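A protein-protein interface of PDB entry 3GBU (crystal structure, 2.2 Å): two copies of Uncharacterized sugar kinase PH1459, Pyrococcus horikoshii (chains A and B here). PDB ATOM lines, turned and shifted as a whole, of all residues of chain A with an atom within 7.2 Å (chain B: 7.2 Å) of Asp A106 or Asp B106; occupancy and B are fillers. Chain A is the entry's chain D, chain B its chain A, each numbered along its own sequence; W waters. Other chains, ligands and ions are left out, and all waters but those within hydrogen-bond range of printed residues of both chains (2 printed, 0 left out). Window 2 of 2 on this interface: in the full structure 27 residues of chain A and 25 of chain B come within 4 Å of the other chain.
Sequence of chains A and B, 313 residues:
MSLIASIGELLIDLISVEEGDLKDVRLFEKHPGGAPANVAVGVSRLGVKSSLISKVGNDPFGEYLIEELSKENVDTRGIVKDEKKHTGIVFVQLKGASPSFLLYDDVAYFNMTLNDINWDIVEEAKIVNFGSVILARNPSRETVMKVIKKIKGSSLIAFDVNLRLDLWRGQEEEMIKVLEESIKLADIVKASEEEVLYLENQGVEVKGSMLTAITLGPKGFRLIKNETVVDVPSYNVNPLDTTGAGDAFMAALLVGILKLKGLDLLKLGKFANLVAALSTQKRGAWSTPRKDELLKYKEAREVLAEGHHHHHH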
ATOM      1  N   LYS A  84       4.668 -20.194 -21.505  1.00  0.00           N
ATOM      2  CA  LYS A  84       4.962 -21.282 -20.584  1.00  0.00           C
ATOM      3  C   LYS A  84       4.860 -20.863 -19.124  1.00  0.00           C
ATOM      4  O   LYS A  84       4.265 -21.566 -18.305  1.00  0.00           O
ATOM      5  CB  LYS A  84       6.364 -21.830 -20.860  1.00  0.00           C
ATOM      6  CG  LYS A  84       6.665 -22.036 -22.339  1.00  0.00           C
ATOM      7  CD  LYS A  84       5.611 -22.914 -23.004  1.00  0.00           C
ATOM      8  CE  LYS A  84       5.876 -23.092 -24.492  1.00  0.00           C
ATOM      9  NZ  LYS A  84       4.801 -23.913 -25.126  1.00  0.00           N
ATOM     10  N   LYS A  85       5.447 -19.716 -18.805  1.00  0.00           N
ATOM     11  CA  LYS A  85       5.436 -19.213 -17.440  1.00  0.00           C
ATOM     12  C   LYS A  85       4.249 -18.285 -17.213  1.00  0.00           C
ATOM     13  O   LYS A  85       3.832 -17.555 -18.114  1.00  0.00           O
ATOM     14  CB  LYS A  85       6.745 -18.467 -17.144  1.00  0.00           C
ATOM     15  CG  LYS A  85       8.014 -19.278 -17.409  1.00  0.00           C
ATOM     16  CD  LYS A  85       7.916 -20.676 -16.819  1.00  0.00           C
ATOM     17  CE  LYS A  85       9.257 -21.383 -16.801  1.00  0.00           C
ATOM     18  NZ  LYS A  85      10.098 -20.908 -15.675  1.00  0.00           N
ATOM     19  N   HIS A  86       3.696 -18.324 -16.009  1.00  0.00           N
ATOM     20  CA  HIS A  86       2.580 -17.459 -15.695  1.00  0.00           C
ATOM     21  C   HIS A  86       3.060 -16.146 -15.100  1.00  0.00           C
ATOM     22  O   HIS A  86       4.194 -16.041 -14.628  1.00  0.00           O
ATOM     23  CB  HIS A  86       1.606 -18.168 -14.757  1.00  0.00           C
ATOM     24  CG  HIS A  86       0.656 -19.074 -15.475  1.00  0.00           C
ATOM     25  ND1 HIS A  86       0.622 -20.436 -15.272  1.00  0.00           N
ATOM     26  CD2 HIS A  86      -0.265 -18.812 -16.435  1.00  0.00           C
ATOM     27  CE1 HIS A  86      -0.278 -20.976 -16.076  1.00  0.00           C
ATOM     28  NE2 HIS A  86      -0.830 -20.011 -16.791  1.00  0.00           N
ATOM     29  N   THR A  87       2.191 -15.145 -15.155  1.00  0.00           N
ATOM     30  CA  THR A  87       2.490 -13.813 -14.649  1.00  0.00           C
ATOM     31  C   THR A  87       3.027 -13.832 -13.224  1.00  0.00           C
ATOM     32  O   THR A  87       2.568 -14.604 -12.380  1.00  0.00           O
ATOM     33  CB  THR A  87       1.234 -12.931 -14.696  1.00  0.00           C
ATOM     34  OG1 THR A  87       0.722 -12.924 -16.034  1.00  0.00           O
ATOM     35  CG2 THR A  87       1.553 -11.500 -14.253  1.00  0.00           C
ATOM     36  N   GLY A  88       4.011 -12.980 -12.971  1.00  0.00           N
ATOM     37  CA  GLY A  88       4.592 -12.891 -11.646  1.00  0.00           C
ATOM     38  C   GLY A  88       3.589 -12.479 -10.580  1.00  0.00           C
ATOM     39  O   GLY A  88       2.643 -11.715 -10.830  1.00  0.00           O
ATOM     40  N   LEU A 103       7.281 -14.397  -2.456  1.00  0.00           N
ATOM     41  CA  LEU A 103       7.367 -14.223  -3.895  1.00  0.00           C
ATOM     42  C   LEU A 103       7.569 -15.537  -4.639  1.00  0.00           C
ATOM     43  O   LEU A 103       8.369 -16.382  -4.234  1.00  0.00           O
ATOM     44  CB  LEU A 103       8.490 -13.228  -4.215  1.00  0.00           C
ATOM     45  CG  LEU A 103       8.744 -12.850  -5.675  1.00  0.00           C
ATOM     46  CD1 LEU A 103       9.252 -11.408  -5.776  1.00  0.00           C
ATOM     47  CD2 LEU A 103       9.747 -13.853  -6.276  1.00  0.00           C
ATOM     48  N   TYR A 104       6.815 -15.716  -5.717  1.00  0.00           N
ATOM     49  CA  TYR A 104       6.924 -16.927  -6.521  1.00  0.00           C
ATOM     50  C   TYR A 104       7.886 -16.619  -7.665  1.00  0.00           C
ATOM     51  O   TYR A 104       7.630 -15.745  -8.484  1.00  0.00           O
ATOM     52  CB  TYR A 104       5.531 -17.352  -7.013  1.00  0.00           C
ATOM     53  CG  TYR A 104       4.742 -18.034  -5.918  1.00  0.00           C
ATOM     54  CD1 TYR A 104       4.329 -17.326  -4.788  1.00  0.00           C
ATOM     55  CD2 TYR A 104       4.508 -19.412  -5.953  1.00  0.00           C
ATOM     56  CE1 TYR A 104       3.711 -17.973  -3.711  1.00  0.00           C
ATOM     57  CE2 TYR A 104       3.895 -20.066  -4.884  1.00  0.00           C
ATOM     58  CZ  TYR A 104       3.505 -19.342  -3.766  1.00  0.00           C
ATOM     59  OH  TYR A 104       2.958 -19.997  -2.687  1.00  0.00           O
ATOM     60  N   ASP A 105       9.004 -17.341  -7.705  1.00  0.00           N
ATOM     61  CA  ASP A 105      10.033 -17.084  -8.707  1.00  0.00           C
ATOM     62  C   ASP A 105       9.989 -17.784 -10.060  1.00  0.00           C
ATOM     63  O   ASP A 105      10.679 -17.349 -10.983  1.00  0.00           O
ATOM     64  CB  ASP A 105      11.416 -17.299  -8.087  1.00  0.00           C
ATOM     65  CG  ASP A 105      11.703 -18.752  -7.803  1.00  0.00           C
ATOM     66  OD1 ASP A 105      10.858 -19.403  -7.153  1.00  0.00           O
ATOM     67  OD2 ASP A 105      12.770 -19.243  -8.228  1.00  0.00           O
ATOM     68  N   ASP A 106       9.223 -18.855 -10.216  1.00  0.00           N
ATOM     69  CA  ASP A 106       9.212 -19.472 -11.537  1.00  0.00           C
ATOM     70  C   ASP A 106       8.142 -18.782 -12.358  1.00  0.00           C
ATOM     71  O   ASP A 106       7.195 -19.413 -12.827  1.00  0.00           O
ATOM     72  CB  ASP A 106       8.938 -20.978 -11.467  1.00  0.00           C
ATOM     73  CG  ASP A 106       9.242 -21.683 -12.791  1.00  0.00           C
ATOM     74  OD1 ASP A 106      10.408 -21.614 -13.240  1.00  0.00           O
ATOM     75  OD2 ASP A 106       8.324 -22.297 -13.388  1.00  0.00           O
ATOM     76  N   VAL A 107       8.301 -17.476 -12.531  1.00  0.00           N
ATOM     77  CA  VAL A 107       7.326 -16.691 -13.269  1.00  0.00           C
ATOM     78  C   VAL A 107       7.872 -16.044 -14.528  1.00  0.00           C
ATOM     79  O   VAL A 107       9.073 -16.053 -14.775  1.00  0.00           O
ATOM     80  CB  VAL A 107       6.702 -15.626 -12.356  1.00  0.00           C
ATOM     81  CG1 VAL A 107       5.941 -16.320 -11.242  1.00  0.00           C
ATOM     82  CG2 VAL A 107       7.794 -14.719 -11.766  1.00  0.00           C
ATOM     83  N   ALA A 108       6.970 -15.469 -15.310  1.00  0.00           N
ATOM     84  CA  ALA A 108       7.308 -14.855 -16.587  1.00  0.00           C
ATOM     85  C   ALA A 108       8.363 -13.748 -16.640  1.00  0.00           C
ATOM     86  O   ALA A 108       9.151 -13.709 -17.590  1.00  0.00           O
ATOM     87  CB  ALA A 108       6.031 -14.372 -17.263  1.00  0.00           C
ATOM     88  N   TYR A 109       8.391 -12.840 -15.667  1.00  0.00           N
ATOM     89  CA  TYR A 109       9.377 -11.765 -15.741  1.00  0.00           C
ATOM     90  C   TYR A 109      10.805 -12.235 -15.475  1.00  0.00           C
ATOM     91  O   TYR A 109      11.758 -11.536 -15.807  1.00  0.00           O
ATOM     92  CB  TYR A 109       8.993 -10.596 -14.815  1.00  0.00           C
ATOM     93  CG  TYR A 109       9.081 -10.872 -13.334  1.00  0.00           C
ATOM     94  CD1 TYR A 109      10.316 -10.910 -12.687  1.00  0.00           C
ATOM     95  CD2 TYR A 109       7.929 -11.083 -12.571  1.00  0.00           C
ATOM     96  CE1 TYR A 109      10.401 -11.149 -11.314  1.00  0.00           C
ATOM     97  CE2 TYR A 109       8.005 -11.325 -11.198  1.00  0.00           C
ATOM     98  CZ  TYR A 109       9.244 -11.355 -10.576  1.00  0.00           C
ATOM     99  OH  TYR A 109       9.331 -11.580  -9.219  1.00  0.00           O
ATOM    100  N   PHE A 110      10.952 -13.423 -14.889  1.00  0.00           N
ATOM    101  CA  PHE A 110      12.278 -13.986 -14.629  1.00  0.00           C
ATOM    102  C   PHE A 110      12.733 -14.864 -15.797  1.00  0.00           C
ATOM    103  O   PHE A 110      13.818 -15.454 -15.752  1.00  0.00           O
ATOM    104  CB  PHE A 110      12.275 -14.853 -13.369  1.00  0.00           C
ATOM    105  CG  PHE A 110      12.525 -14.097 -12.094  1.00  0.00           C
ATOM    106  CD1 PHE A 110      13.560 -13.167 -12.006  1.00  0.00           C
ATOM    107  CD2 PHE A 110      11.773 -14.369 -10.956  1.00  0.00           C
ATOM    108  CE1 PHE A 110      13.837 -12.526 -10.798  1.00  0.00           C
ATOM    109  CE2 PHE A 110      12.046 -13.737  -9.753  1.00  0.00           C
ATOM    110  CZ  PHE A 110      13.080 -12.816  -9.675  1.00  0.00           C
ATOM    111  N   ASN A 111      11.908 -14.948 -16.837  1.00  0.00           N
ATOM    112  CA  ASN A 111      12.214 -15.789 -17.989  1.00  0.00           C
ATOM    113  C   ASN A 111      12.444 -15.040 -19.302  1.00  0.00           C
ATOM    114  O   ASN A 111      12.152 -15.563 -20.377  1.00  0.00           O
ATOM    115  CB  ASN A 111      11.084 -16.808 -18.169  1.00  0.00           C
ATOM    116  CG  ASN A 111      11.440 -17.912 -19.140  1.00  0.00           C
ATOM    117  OD1 ASN A 111      12.525 -18.485 -19.066  1.00  0.00           O
ATOM    118  ND2 ASN A 111      10.521 -18.225 -20.053  1.00  0.00           N
ATOM    119  N   ARG A 137      17.240 -14.137 -10.916  1.00  0.00           N
ATOM    120  CA  ARG A 137      17.087 -15.385 -11.654  1.00  0.00           C
ATOM    121  C   ARG A 137      17.369 -15.225 -13.144  1.00  0.00           C
ATOM    122  O   ARG A 137      17.096 -14.177 -13.731  1.00  0.00           O
ATOM    123  CB  ARG A 137      15.655 -15.926 -11.487  1.00  0.00           C
ATOM    124  CG  ARG A 137      15.191 -16.180 -10.055  1.00  0.00           C
ATOM    125  CD  ARG A 137      15.624 -17.549  -9.532  1.00  0.00           C
ATOM    126  NE  ARG A 137      15.138 -17.776  -8.169  1.00  0.00           N
ATOM    127  CZ  ARG A 137      15.540 -17.082  -7.107  1.00  0.00           C
ATOM    128  NH1 ARG A 137      16.446 -16.117  -7.253  1.00  0.00           N
ATOM    129  NH2 ARG A 137      15.026 -17.334  -5.904  1.00  0.00           N
ATOM    130  N   LYS B  85      11.070 -25.154  -3.728  1.00  0.00           N
ATOM    131  CA  LYS B  85       9.758 -24.822  -4.271  1.00  0.00           C
ATOM    132  C   LYS B  85       8.763 -24.285  -3.239  1.00  0.00           C
ATOM    133  O   LYS B  85       8.720 -24.742  -2.099  1.00  0.00           O
ATOM    134  CB  LYS B  85       9.173 -26.055  -4.967  1.00  0.00           C
ATOM    135  CG  LYS B  85      10.089 -26.656  -6.027  1.00  0.00           C
ATOM    136  CD  LYS B  85      10.427 -25.634  -7.105  1.00  0.00           C
ATOM    137  CE  LYS B  85      11.383 -26.208  -8.151  1.00  0.00           C
ATOM    138  NZ  LYS B  85      10.807 -27.365  -8.869  1.00  0.00           N
ATOM    139  N   HIS B  86       7.961 -23.312  -3.659  1.00  0.00           N
ATOM    140  CA  HIS B  86       6.959 -22.705  -2.789  1.00  0.00           C
ATOM    141  C   HIS B  86       5.661 -23.505  -2.790  1.00  0.00           C
ATOM    142  O   HIS B  86       5.415 -24.313  -3.688  1.00  0.00           O
ATOM    143  CB  HIS B  86       6.671 -21.280  -3.238  1.00  0.00           C
ATOM    144  CG  HIS B  86       7.872 -20.392  -3.211  1.00  0.00           C
ATOM    145  ND1 HIS B  86       8.376 -19.858  -2.044  1.00  0.00           N
ATOM    146  CD2 HIS B  86       8.674 -19.949  -4.208  1.00  0.00           C
ATOM    147  CE1 HIS B  86       9.435 -19.120  -2.326  1.00  0.00           C
ATOM    148  NE2 HIS B  86       9.638 -19.159  -3.631  1.00  0.00           N
ATOM    149  N   THR B  87       4.844 -23.265  -1.767  1.00  0.00           N
ATOM    150  CA  THR B  87       3.557 -23.935  -1.589  1.00  0.00           C
ATOM    151  C   THR B  87       2.662 -23.756  -2.825  1.00  0.00           C
ATOM    152  O   THR B  87       2.630 -22.686  -3.431  1.00  0.00           O
ATOM    153  CB  THR B  87       2.831 -23.362  -0.335  1.00  0.00           C
ATOM    154  OG1 THR B  87       3.653 -23.560   0.825  1.00  0.00           O
ATOM    155  CG2 THR B  87       1.473 -24.049  -0.117  1.00  0.00           C
ATOM    156  N   GLY B  88       1.945 -24.808  -3.205  1.00  0.00           N
ATOM    157  CA  GLY B  88       1.067 -24.696  -4.355  1.00  0.00           C
ATOM    158  C   GLY B  88      -0.025 -23.645  -4.169  1.00  0.00           C
ATOM    159  O   GLY B  88      -0.508 -23.422  -3.059  1.00  0.00           O
ATOM    160  N   LEU B 103      -3.682 -21.822 -12.288  1.00  0.00           N
ATOM    161  CA  LEU B 103      -2.857 -22.650 -11.418  1.00  0.00           C
ATOM    162  C   LEU B 103      -1.360 -22.494 -11.691  1.00  0.00           C
ATOM    163  O   LEU B 103      -0.923 -22.558 -12.839  1.00  0.00           O
ATOM    164  CB  LEU B 103      -3.269 -24.125 -11.572  1.00  0.00           C
ATOM    165  CG  LEU B 103      -2.590 -25.167 -10.671  1.00  0.00           C
ATOM    166  CD1 LEU B 103      -3.493 -26.379 -10.496  1.00  0.00           C
ATOM    167  CD2 LEU B 103      -1.246 -25.567 -11.279  1.00  0.00           C
ATOM    168  N   TYR B 104      -0.580 -22.283 -10.633  1.00  0.00           N
ATOM    169  CA  TYR B 104       0.868 -22.150 -10.778  1.00  0.00           C
ATOM    170  C   TYR B 104       1.467 -23.534 -10.614  1.00  0.00           C
ATOM    171  O   TYR B 104       1.321 -24.161  -9.569  1.00  0.00           O
ATOM    172  CB  TYR B 104       1.422 -21.161  -9.749  1.00  0.00           C
ATOM    173  CG  TYR B 104       1.172 -19.734 -10.173  1.00  0.00           C
ATOM    174  CD1 TYR B 104      -0.130 -19.234 -10.261  1.00  0.00           C
ATOM    175  CD2 TYR B 104       2.221 -18.919 -10.598  1.00  0.00           C
ATOM    176  CE1 TYR B 104      -0.380 -17.964 -10.773  1.00  0.00           C
ATOM    177  CE2 TYR B 104       1.982 -17.649 -11.111  1.00  0.00           C
ATOM    178  CZ  TYR B 104       0.683 -17.181 -11.199  1.00  0.00           C
ATOM    179  OH  TYR B 104       0.439 -15.940 -11.733  1.00  0.00           O
ATOM    180  N   ASP B 105       2.154 -24.008 -11.647  1.00  0.00           N
ATOM    181  CA  ASP B 105       2.680 -25.370 -11.628  1.00  0.00           C
ATOM    182  C   ASP B 105       4.072 -25.697 -11.077  1.00  0.00           C
ATOM    183  O   ASP B 105       4.319 -26.834 -10.681  1.00  0.00           O
ATOM    184  CB  ASP B 105       2.523 -25.977 -13.026  1.00  0.00           C
ATOM    185  CG  ASP B 105       3.394 -25.293 -14.066  1.00  0.00           C
ATOM    186  OD1 ASP B 105       3.661 -24.077 -13.938  1.00  0.00           O
ATOM    187  OD2 ASP B 105       3.797 -25.978 -15.024  1.00  0.00           O
ATOM    188  N   ASP B 106       4.990 -24.744 -11.035  1.00  0.00           N
ATOM    189  CA  ASP B 106       6.294 -25.087 -10.488  1.00  0.00           C
ATOM    190  C   ASP B 106       6.200 -24.819  -8.988  1.00  0.00           C
ATOM    191  O   ASP B 106       6.657 -23.788  -8.503  1.00  0.00           O
ATOM    192  CB  ASP B 106       7.393 -24.229 -11.122  1.00  0.00           C
ATOM    193  CG  ASP B 106       8.775 -24.831 -10.941  1.00  0.00           C
ATOM    194  OD1 ASP B 106       9.747 -24.258 -11.475  1.00  0.00           O
ATOM    195  OD2 ASP B 106       8.888 -25.881 -10.264  1.00  0.00           O
ATOM    196  N   VAL B 107       5.582 -25.754  -8.271  1.00  0.00           N
ATOM    197  CA  VAL B 107       5.373 -25.630  -6.839  1.00  0.00           C
ATOM    198  C   VAL B 107       5.664 -26.951  -6.114  1.00  0.00           C
ATOM    199  O   VAL B 107       5.824 -27.992  -6.735  1.00  0.00           O
ATOM    200  CB  VAL B 107       3.915 -25.153  -6.536  1.00  0.00           C
ATOM    201  CG1 VAL B 107       3.697 -23.769  -7.123  1.00  0.00           C
ATOM    202  CG2 VAL B 107       2.888 -26.131  -7.128  1.00  0.00           C
ATOM    203  N   ALA B 108       5.705 -26.893  -4.792  1.00  0.00           N
ATOM    204  CA  ALA B 108       6.031 -28.044  -3.963  1.00  0.00           C
ATOM    205  C   ALA B 108       5.344 -29.394  -4.195  1.00  0.00           C
ATOM    206  O   ALA B 108       6.033 -30.420  -4.258  1.00  0.00           O
ATOM    207  CB  ALA B 108       5.900 -27.657  -2.512  1.00  0.00           C
ATOM    208  N   TYR B 109       4.015 -29.425  -4.318  1.00  0.00           N
ATOM    209  CA  TYR B 109       3.348 -30.715  -4.481  1.00  0.00           C
ATOM    210  C   TYR B 109       3.679 -31.450  -5.783  1.00  0.00           C
ATOM    211  O   TYR B 109       3.500 -32.663  -5.870  1.00  0.00           O
ATOM    212  CB  TYR B 109       1.816 -30.584  -4.269  1.00  0.00           C
ATOM    213  CG  TYR B 109       1.042 -29.824  -5.334  1.00  0.00           C
ATOM    214  CD1 TYR B 109       0.730 -30.420  -6.555  1.00  0.00           C
ATOM    215  CD2 TYR B 109       0.628 -28.509  -5.122  1.00  0.00           C
ATOM    216  CE1 TYR B 109       0.027 -29.728  -7.545  1.00  0.00           C
ATOM    217  CE2 TYR B 109      -0.076 -27.801  -6.115  1.00  0.00           C
ATOM    218  CZ  TYR B 109      -0.366 -28.422  -7.321  1.00  0.00           C
ATOM    219  OH  TYR B 109      -1.018 -27.743  -8.324  1.00  0.00           O
ATOM    220  N   PHE B 110       4.179 -30.726  -6.781  1.00  0.00           N
ATOM    221  CA  PHE B 110       4.563 -31.343  -8.053  1.00  0.00           C
ATOM    222  C   PHE B 110       6.035 -31.794  -8.007  1.00  0.00           C
ATOM    223  O   PHE B 110       6.532 -32.411  -8.947  1.00  0.00           O
ATOM    224  CB  PHE B 110       4.395 -30.354  -9.216  1.00  0.00           C
ATOM    225  CG  PHE B 110       2.986 -30.258  -9.758  1.00  0.00           C
ATOM    226  CD1 PHE B 110       2.263 -31.404 -10.071  1.00  0.00           C
ATOM    227  CD2 PHE B 110       2.428 -29.014 -10.054  1.00  0.00           C
ATOM    228  CE1 PHE B 110       1.017 -31.319 -10.676  1.00  0.00           C
ATOM    229  CE2 PHE B 110       1.173 -28.915 -10.665  1.00  0.00           C
ATOM    230  CZ  PHE B 110       0.467 -30.072 -10.980  1.00  0.00           C
ATOM    231  N   ASN B 111       6.724 -31.486  -6.912  1.00  0.00           N
ATOM    232  CA  ASN B 111       8.138 -31.831  -6.770  1.00  0.00           C
ATOM    233  C   ASN B 111       8.447 -32.983  -5.809  1.00  0.00           C
ATOM    234  O   ASN B 111       9.498 -32.986  -5.165  1.00  0.00           O
ATOM    235  CB  ASN B 111       8.918 -30.583  -6.329  1.00  0.00           C
ATOM    236  CG  ASN B 111      10.402 -30.709  -6.579  1.00  0.00           C
ATOM    237  OD1 ASN B 111      10.814 -31.212  -7.616  1.00  0.00           O
ATOM    238  ND2 ASN B 111      11.210 -30.244  -5.642  1.00  0.00           N
ATOM    239  N   ARG B 137       2.493 -33.383 -13.477  1.00  0.00           N
ATOM    240  CA  ARG B 137       3.901 -33.021 -13.611  1.00  0.00           C
ATOM    241  C   ARG B 137       4.837 -33.991 -12.887  1.00  0.00           C
ATOM    242  O   ARG B 137       4.449 -34.661 -11.925  1.00  0.00           O
ATOM    243  CB  ARG B 137       4.146 -31.613 -13.048  1.00  0.00           C
ATOM    244  CG  ARG B 137       3.316 -30.490 -13.672  1.00  0.00           C
ATOM    245  CD  ARG B 137       4.021 -29.834 -14.849  1.00  0.00           C
ATOM    246  NE  ARG B 137       3.229 -28.725 -15.382  1.00  0.00           N
ATOM    247  CZ  ARG B 137       2.069 -28.870 -16.020  1.00  0.00           C
ATOM    248  NH1 ARG B 137       1.565 -30.075 -16.218  1.00  0.00           N
ATOM    249  NH2 ARG B 137       1.397 -27.804 -16.444  1.00  0.00           N
ATOM    250  N   ASN B 138       6.068 -34.072 -13.382  1.00  0.00           N
ATOM    251  CA  ASN B 138       7.101 -34.879 -12.755  1.00  0.00           C
ATOM    252  C   ASN B 138       7.843 -33.873 -11.885  1.00  0.00           C
ATOM    253  O   ASN B 138       7.735 -32.667 -12.101  1.00  0.00           O
ATOM    254  CB  ASN B 138       8.055 -35.471 -13.804  1.00  0.00           C
ATOM    255  CG  ASN B 138       7.622 -36.846 -14.270  1.00  0.00           C
ATOM    256  OD1 ASN B 138       7.685 -37.164 -15.456  1.00  0.00           O
ATOM    257  ND2 ASN B 138       7.184 -37.672 -13.334  1.00  0.00           N
HETATM  258  O   HOH W   1      11.208 -16.605  -2.957  1.00  0.00           O
HETATM  259  O   HOH W   2       2.674 -21.446 -14.107  1.00  0.00           O
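The side-chain hydroxyl (OH) of Tyr A104 is in hydrogen-bond range of the backbone carbonyl oxygen (O) of Thr B87 (2.8 Å).
NE2 of His B86 sits at hydrogen-bond distance from O of Leu A103, at 3.1 Å.
O of Thr A87 lies within hydrogen-bond range of OH of Tyr B104 (2.6 Å).
The side-chain carboxylate (OD1) of Asp B106 sits close to the side-chain carboxylate (OD2) of Asp A106, 3.1 Å away.
OD1 of Asp A106 lies within salt-bridge range of NZ of Lys A85.
OD2 of Asp A105 lies within salt-bridge range of NE of Arg A137.
N of Ala A108 lies within hydrogen-bond range of O of His A86.
The backbone carbonyl oxygen (O) of His B86 is in hydrogen-bond range of the backbone NH (N) of Ala B108, 2.8 Å away.
The side-chain carboxylate (OD2) of Asp B106 is in salt-bridge range of the side-chain amino group (NZ) of Lys B85, at 2.8 Å.
Among the printed residues, merely in contact across the chains: His A86 with Leu B103 (3.6 Å), His A86 with Tyr B104 (3.7 Å), Tyr A104 with His B86 (3.4 Å) and Asp A105 with His B86 (3.7 Å).
Lys A84 touches none of the printed residues of chain B.
Printed residues of chain B within 4 Å of Thr A87: Tyr B104.
Printed residues of chain B within 4 Å of Leu A103: His B86 (3.1 Å).
Of the printed residues of chain A, Leu B103 touches His A86 (3.6 Å).
Of the printed residues of chain A, Asp B106 touches Asp A106 (2.9 Å).
The nearest residue of chain B that does not touch Asp A106 is Asp B105 (5.0 Å).
Of the 15 printed residues of chain B, 5 touch a printed residue of chain A.
Printed residues of chain B that touch a printed residue of chain A: His B86, Thr B87, Leu B103, Tyr B104 and Asp B106.
Among the printed residues, 8 pairs touch across the chains.
Among the printed residues, no Asp or Glu carboxylate lies within 4 Å of a Lys or Arg side-chain nitrogen of the other chain.
His A86 touches Leu B103, and with the chains exchanged Leu A103 touches His B86.
His A86 touches Tyr B104, and with the chains exchanged Tyr A104 touches His B86.
Thr A87 touches Tyr B104, and with the chains exchanged Tyr A104 touches Thr B87.
Asp A105 touches His B86, but with the chains exchanged His A86 does not touch Asp B105 (4.9 Å).
Of the 8 pairs that touch across the chains among the printed residues, 7 have their exchanged pair printed and touching as well.
Water W2 lies within hydrogen-bond range of a ring nitrogen (ND1) of His A86 and the side-chain carboxylate (OD1) of Asp B105.
Water W1 lies within hydrogen-bond range of NE2 of His B86 and O of Leu A103.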
